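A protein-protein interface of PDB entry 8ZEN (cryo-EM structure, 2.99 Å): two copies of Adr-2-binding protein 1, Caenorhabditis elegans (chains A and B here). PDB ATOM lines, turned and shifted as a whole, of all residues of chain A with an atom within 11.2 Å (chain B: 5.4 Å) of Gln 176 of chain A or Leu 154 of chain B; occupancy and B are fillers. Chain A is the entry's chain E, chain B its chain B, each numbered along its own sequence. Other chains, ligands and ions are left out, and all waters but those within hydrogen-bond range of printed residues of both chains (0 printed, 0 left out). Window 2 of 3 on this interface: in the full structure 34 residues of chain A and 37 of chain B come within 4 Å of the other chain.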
ATOM      1  N   LEU A 167      22.682  28.225   9.546  1.00  0.00           N
ATOM      2  CA  LEU A 167      21.768  28.378   8.409  1.00  0.00           C
ATOM      3  C   LEU A 167      20.388  27.808   8.712  1.00  0.00           C
ATOM      4  O   LEU A 167      19.431  28.088   7.982  1.00  0.00           O
ATOM      5  CB  LEU A 167      22.295  27.757   7.110  1.00  0.00           C
ATOM      6  CG  LEU A 167      23.721  27.907   6.583  1.00  0.00           C
ATOM      7  CD1 LEU A 167      24.618  26.957   7.267  1.00  0.00           C
ATOM      8  CD2 LEU A 167      23.806  27.716   5.088  1.00  0.00           C
ATOM      9  N   GLN A 170      18.957  30.819  11.214  1.00  0.00           N
ATOM     10  CA  GLN A 170      18.894  32.126  10.575  1.00  0.00           C
ATOM     11  C   GLN A 170      17.584  32.296   9.810  1.00  0.00           C
ATOM     12  O   GLN A 170      16.900  31.325   9.476  1.00  0.00           O
ATOM     13  CB  GLN A 170      20.129  32.322   9.679  1.00  0.00           C
ATOM     14  CG  GLN A 170      20.144  31.688   8.272  1.00  0.00           C
ATOM     15  CD  GLN A 170      19.085  32.220   7.333  1.00  0.00           C
ATOM     16  OE1 GLN A 170      18.909  33.429   7.213  1.00  0.00           O
ATOM     17  NE2 GLN A 170      18.375  31.321   6.662  1.00  0.00           N
ATOM     18  N   ASP A 171      17.238  33.555   9.537  1.00  0.00           N
ATOM     19  CA  ASP A 171      15.956  33.905   8.936  1.00  0.00           C
ATOM     20  C   ASP A 171      16.094  34.418   7.508  1.00  0.00           C
ATOM     21  O   ASP A 171      15.280  34.053   6.653  1.00  0.00           O
ATOM     22  CB  ASP A 171      15.244  34.935   9.841  1.00  0.00           C
ATOM     23  CG  ASP A 171      14.043  35.644   9.179  1.00  0.00           C
ATOM     24  OD1 ASP A 171      14.083  36.060   8.005  1.00  0.00           O
ATOM     25  OD2 ASP A 171      13.046  35.864   9.901  1.00  0.00           O
ATOM     26  N   ASN A 172      17.108  35.233   7.222  1.00  0.00           N
ATOM     27  CA  ASN A 172      17.247  35.885   5.917  1.00  0.00           C
ATOM     28  C   ASN A 172      17.601  34.827   4.880  1.00  0.00           C
ATOM     29  O   ASN A 172      18.758  34.434   4.726  1.00  0.00           O
ATOM     30  CB  ASN A 172      18.297  36.986   5.972  1.00  0.00           C
ATOM     31  CG  ASN A 172      18.680  37.494   4.597  1.00  0.00           C
ATOM     32  OD1 ASN A 172      17.849  37.556   3.691  1.00  0.00           O
ATOM     33  ND2 ASN A 172      19.948  37.856   4.432  1.00  0.00           N
ATOM     34  N   ASP A 173      16.591  34.381   4.140  1.00  0.00           N
ATOM     35  CA  ASP A 173      16.761  33.335   3.135  1.00  0.00           C
ATOM     36  C   ASP A 173      16.868  33.901   1.728  1.00  0.00           C
ATOM     37  O   ASP A 173      16.339  33.327   0.772  1.00  0.00           O
ATOM     38  CB  ASP A 173      15.617  32.334   3.241  1.00  0.00           C
ATOM     39  CG  ASP A 173      15.984  31.125   4.080  1.00  0.00           C
ATOM     40  OD1 ASP A 173      17.171  30.993   4.443  1.00  0.00           O
ATOM     41  OD2 ASP A 173      15.087  30.316   4.392  1.00  0.00           O
ATOM     42  N   SER A 174      17.546  35.044   1.582  1.00  0.00           N
ATOM     43  CA  SER A 174      17.774  35.626   0.263  1.00  0.00           C
ATOM     44  C   SER A 174      18.706  34.773  -0.587  1.00  0.00           C
ATOM     45  O   SER A 174      18.823  35.016  -1.794  1.00  0.00           O
ATOM     46  CB  SER A 174      18.344  37.036   0.404  1.00  0.00           C
ATOM     47  OG  SER A 174      19.718  36.995   0.745  1.00  0.00           O
ATOM     48  N   ASP A 175      19.366  33.781   0.010  1.00  0.00           N
ATOM     49  CA  ASP A 175      20.137  32.791  -0.734  1.00  0.00           C
ATOM     50  C   ASP A 175      19.187  31.846  -1.459  1.00  0.00           C
ATOM     51  O   ASP A 175      19.619  30.954  -2.196  1.00  0.00           O
ATOM     52  CB  ASP A 175      21.060  32.017   0.207  1.00  0.00           C
ATOM     53  CG  ASP A 175      22.124  31.232  -0.531  1.00  0.00           C
ATOM     54  OD1 ASP A 175      22.672  31.757  -1.523  1.00  0.00           O
ATOM     55  OD2 ASP A 175      22.414  30.089  -0.118  1.00  0.00           O
ATOM     56  N   GLN A 176      17.888  32.043  -1.238  1.00  0.00           N
ATOM     57  CA  GLN A 176      16.828  31.265  -1.874  1.00  0.00           C
ATOM     58  C   GLN A 176      16.909  29.795  -1.467  1.00  0.00           C
ATOM     59  O   GLN A 176      16.861  28.885  -2.297  1.00  0.00           O
ATOM     60  CB  GLN A 176      16.851  31.439  -3.393  1.00  0.00           C
ATOM     61  CG  GLN A 176      15.533  31.104  -4.064  1.00  0.00           C
ATOM     62  CD  GLN A 176      15.579  31.294  -5.560  1.00  0.00           C
ATOM     63  OE1 GLN A 176      16.650  31.307  -6.164  1.00  0.00           O
ATOM     64  NE2 GLN A 176      14.414  31.418  -6.170  1.00  0.00           N
ATOM     65  N   PHE A 177      17.053  29.575  -0.162  1.00  0.00           N
ATOM     66  CA  PHE A 177      16.882  28.289   0.509  1.00  0.00           C
ATOM     67  C   PHE A 177      17.930  27.257   0.122  1.00  0.00           C
ATOM     68  O   PHE A 177      17.817  26.093   0.519  1.00  0.00           O
ATOM     69  CB  PHE A 177      15.479  27.723   0.264  1.00  0.00           C
ATOM     70  CG  PHE A 177      14.379  28.695   0.570  1.00  0.00           C
ATOM     71  CD1 PHE A 177      13.998  28.942   1.875  1.00  0.00           C
ATOM     72  CD2 PHE A 177      13.725  29.362  -0.451  1.00  0.00           C
ATOM     73  CE1 PHE A 177      12.987  29.839   2.157  1.00  0.00           C
ATOM     74  CE2 PHE A 177      12.715  30.258  -0.175  1.00  0.00           C
ATOM     75  CZ  PHE A 177      12.345  30.495   1.131  1.00  0.00           C
ATOM     76  N   VAL A 178      18.955  27.646  -0.639  1.00  0.00           N
ATOM     77  CA  VAL A 178      20.056  26.726  -0.913  1.00  0.00           C
ATOM     78  C   VAL A 178      20.776  26.373   0.380  1.00  0.00           C
ATOM     79  O   VAL A 178      21.085  25.205   0.643  1.00  0.00           O
ATOM     80  CB  VAL A 178      21.018  27.331  -1.951  1.00  0.00           C
ATOM     81  CG1 VAL A 178      22.427  26.805  -1.746  1.00  0.00           C
ATOM     82  CG2 VAL A 178      20.543  26.993  -3.341  1.00  0.00           C
ATOM     83  N   GLY A 179      21.041  27.377   1.213  1.00  0.00           N
ATOM     84  CA  GLY A 179      21.716  27.117   2.471  1.00  0.00           C
ATOM     85  C   GLY A 179      20.883  26.283   3.425  1.00  0.00           C
ATOM     86  O   GLY A 179      21.393  25.362   4.069  1.00  0.00           O
ATOM     87  N   TYR A 180      19.590  26.595   3.531  1.00  0.00           N
ATOM     88  CA  TYR A 180      18.721  25.821   4.410  1.00  0.00           C
ATOM     89  C   TYR A 180      18.604  24.379   3.932  1.00  0.00           C
ATOM     90  O   TYR A 180      18.638  23.445   4.739  1.00  0.00           O
ATOM     91  CB  TYR A 180      17.343  26.471   4.499  1.00  0.00           C
ATOM     92  CG  TYR A 180      16.518  25.951   5.651  1.00  0.00           C
ATOM     93  CD1 TYR A 180      16.722  26.417   6.939  1.00  0.00           C
ATOM     94  CD2 TYR A 180      15.542  24.986   5.450  1.00  0.00           C
ATOM     95  CE1 TYR A 180      15.977  25.943   7.994  1.00  0.00           C
ATOM     96  CE2 TYR A 180      14.791  24.506   6.501  1.00  0.00           C
ATOM     97  CZ  TYR A 180      15.013  24.988   7.771  1.00  0.00           C
ATOM     98  OH  TYR A 180      14.269  24.517   8.826  1.00  0.00           O
ATOM     99  N   ALA A 181      18.469  24.179   2.620  1.00  0.00           N
ATOM    100  CA  ALA A 181      18.398  22.823   2.088  1.00  0.00           C
ATOM    101  C   ALA A 181      19.701  22.072   2.318  1.00  0.00           C
ATOM    102  O   ALA A 181      19.689  20.873   2.615  1.00  0.00           O
ATOM    103  CB  ALA A 181      18.059  22.858   0.602  1.00  0.00           C
ATOM    104  N   ALA A 182      20.837  22.757   2.172  1.00  0.00           N
ATOM    105  CA  ALA A 182      22.123  22.121   2.437  1.00  0.00           C
ATOM    106  C   ALA A 182      22.228  21.699   3.895  1.00  0.00           C
ATOM    107  O   ALA A 182      22.699  20.599   4.205  1.00  0.00           O
ATOM    108  CB  ALA A 182      23.263  23.066   2.063  1.00  0.00           C
ATOM    109  N   ALA A 183      21.785  22.564   4.809  1.00  0.00           N
ATOM    110  CA  ALA A 183      21.798  22.214   6.226  1.00  0.00           C
ATOM    111  C   ALA A 183      20.879  21.034   6.511  1.00  0.00           C
ATOM    112  O   ALA A 183      21.219  20.146   7.303  1.00  0.00           O
ATOM    113  CB  ALA A 183      21.399  23.423   7.067  1.00  0.00           C
ATOM    114  N   GLN B 152      20.798  36.644 -10.911  1.00  0.00           N
ATOM    115  CA  GLN B 152      20.837  35.493 -11.802  1.00  0.00           C
ATOM    116  C   GLN B 152      19.939  34.416 -11.219  1.00  0.00           C
ATOM    117  O   GLN B 152      20.054  34.077 -10.038  1.00  0.00           O
ATOM    118  CB  GLN B 152      22.299  35.031 -11.944  1.00  0.00           C
ATOM    119  CG  GLN B 152      22.710  33.961 -12.999  1.00  0.00           C
ATOM    120  CD  GLN B 152      21.891  32.683 -13.061  1.00  0.00           C
ATOM    121  OE1 GLN B 152      21.266  32.273 -12.094  1.00  0.00           O
ATOM    122  NE2 GLN B 152      21.915  32.036 -14.219  1.00  0.00           N
ATOM    123  N   ILE B 153      19.041  33.877 -12.045  1.00  0.00           N
ATOM    124  CA  ILE B 153      17.968  33.040 -11.517  1.00  0.00           C
ATOM    125  C   ILE B 153      18.582  31.764 -10.955  1.00  0.00           C
ATOM    126  O   ILE B 153      18.995  30.857 -11.685  1.00  0.00           O
ATOM    127  CB  ILE B 153      16.867  32.787 -12.574  1.00  0.00           C
ATOM    128  CG1 ILE B 153      15.582  32.265 -11.916  1.00  0.00           C
ATOM    129  CG2 ILE B 153      17.344  31.945 -13.767  1.00  0.00           C
ATOM    130  CD1 ILE B 153      15.203  32.988 -10.643  1.00  0.00           C
ATOM    131  N   LEU B 154      18.660  31.714  -9.629  1.00  0.00           N
ATOM    132  CA  LEU B 154      19.527  30.744  -8.969  1.00  0.00           C
ATOM    133  C   LEU B 154      19.130  29.291  -9.200  1.00  0.00           C
ATOM    134  O   LEU B 154      20.014  28.496  -9.564  1.00  0.00           O
ATOM    135  CB  LEU B 154      19.587  31.070  -7.473  1.00  0.00           C
ATOM    136  CG  LEU B 154      20.821  30.622  -6.695  1.00  0.00           C
ATOM    137  CD1 LEU B 154      21.294  31.725  -5.764  1.00  0.00           C
ATOM    138  CD2 LEU B 154      20.483  29.377  -5.912  1.00  0.00           C
ATOM    139  N   PRO B 155      17.874  28.873  -9.032  1.00  0.00           N
ATOM    140  CA  PRO B 155      17.595  27.436  -9.054  1.00  0.00           C
ATOM    141  C   PRO B 155      17.244  26.898 -10.429  1.00  0.00           C
ATOM    142  O   PRO B 155      16.746  27.628 -11.291  1.00  0.00           O
ATOM    143  CB  PRO B 155      16.409  27.313  -8.095  1.00  0.00           C
ATOM    144  CG  PRO B 155      15.679  28.626  -8.241  1.00  0.00           C
ATOM    145  CD  PRO B 155      16.632  29.641  -8.838  1.00  0.00           C
ATOM    146  N   ARG B 156      17.516  25.616 -10.641  1.00  0.00           N
ATOM    147  CA  ARG B 156      16.931  24.906 -11.767  1.00  0.00           C
ATOM    148  C   ARG B 156      15.548  24.411 -11.373  1.00  0.00           C
ATOM    149  O   ARG B 156      15.418  23.467 -10.588  1.00  0.00           O
ATOM    150  CB  ARG B 156      17.821  23.740 -12.188  1.00  0.00           C
ATOM    151  CG  ARG B 156      19.101  24.149 -12.890  1.00  0.00           C
ATOM    152  CD  ARG B 156      19.926  22.926 -13.254  1.00  0.00           C
ATOM    153  NE  ARG B 156      20.115  22.036 -12.115  1.00  0.00           N
ATOM    154  CZ  ARG B 156      20.864  22.317 -11.057  1.00  0.00           C
ATOM    155  NH1 ARG B 156      21.553  23.443 -10.974  1.00  0.00           N
ATOM    156  NH2 ARG B 156      20.932  21.439 -10.060  1.00  0.00           N
ATOM    157  N   ALA B 185      13.895  22.441  -0.884  1.00  0.00           N
ATOM    158  CA  ALA B 185      14.310  23.781  -1.282  1.00  0.00           C
ATOM    159  C   ALA B 185      13.353  24.375  -2.303  1.00  0.00           C
ATOM    160  O   ALA B 185      12.930  25.529  -2.176  1.00  0.00           O
ATOM    161  CB  ALA B 185      15.730  23.747  -1.843  1.00  0.00           C
ATOM    162  N   ARG B 189      11.157  27.576  -2.196  1.00  0.00           N
ATOM    163  CA  ARG B 189      11.368  28.664  -3.145  1.00  0.00           C
ATOM    164  C   ARG B 189      10.048  29.203  -3.682  1.00  0.00           C
ATOM    165  O   ARG B 189       9.871  30.420  -3.808  1.00  0.00           O
ATOM    166  CB  ARG B 189      12.256  28.193  -4.294  1.00  0.00           C
ATOM    167  CG  ARG B 189      13.723  28.087  -3.935  1.00  0.00           C
ATOM    168  CD  ARG B 189      14.514  27.424  -5.043  1.00  0.00           C
ATOM    169  NE  ARG B 189      15.867  27.095  -4.617  1.00  0.00           N
ATOM    170  CZ  ARG B 189      16.505  25.983  -4.945  1.00  0.00           C
ATOM    171  NH1 ARG B 189      15.950  25.073  -5.726  1.00  0.00           N
ATOM    172  NH2 ARG B 189      17.734  25.779  -4.483  1.00  0.00           N
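CB of Leu 154 of chain B touches OE1 of Gln 176 of chain A (3.2 Å). Gln 176 of chain A touches Pro 155 of chain B. Phe 177 of chain A touches Ala 185 of chain B. Phe 177 of chain A touches Arg 189 of chain B. Val 178 of chain A touches Leu 154 of chain B (CG2 to CD2, 3.5 Å). CG2 of Val 178 of chain A touches NH2 of Arg 189 of chain B, 3.3 Å away. CB of Ala 181 of chain A touches CB of Ala 185 of chain B, at 3.5 Å.
No position is printed for both chains. Of the 8 pairs that touch across the chains among the printed residues, none has its exchanged pair printed and touching as well.
Of chain B, only Leu 154, Pro 155 and Arg 189 come within 4 Å of Gln 176 of chain A. Of the printed residues of chain B, Val 178 of chain A touches Leu 154 (3.5 Å) and Arg 189 (3.3 Å). Printed residues of chain B within 4 Å of Ala 181 of chain A: Ala 185. No residue of chain A comes within 4 Å of Gln 152 of chain B. Of the printed residues of chain A, Leu 154 of chain B touches Gln 176 (3.2 Å) and Val 178 (3.5 Å). Printed residues of chain A within 4 Å of Ala 185 of chain B: Phe 177 and Ala 181. Of chain A, only Gln 176 (3.1 Å), Phe 177 (3.6 Å) and Val 178 (3.3 Å) come within 4 Å of Arg 189 of chain B. The nearest printed residue of chain B that does not touch Phe 177 of chain A is Leu 154 of chain B (6.7 Å).
Hydrophobic or aromatic side chains of chain B within 4 Å of the printed part of chain A: Leu 154, Pro 155 and Ala 185. Among the printed residues, no Asp or Glu carboxylate lies within 4 Å of a Lys or Arg side-chain nitrogen of the other chain.
NE of Arg 189 of chain B lies within hydrogen-bond range of O of Gln 176 of chain A, 3.1 Å away.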
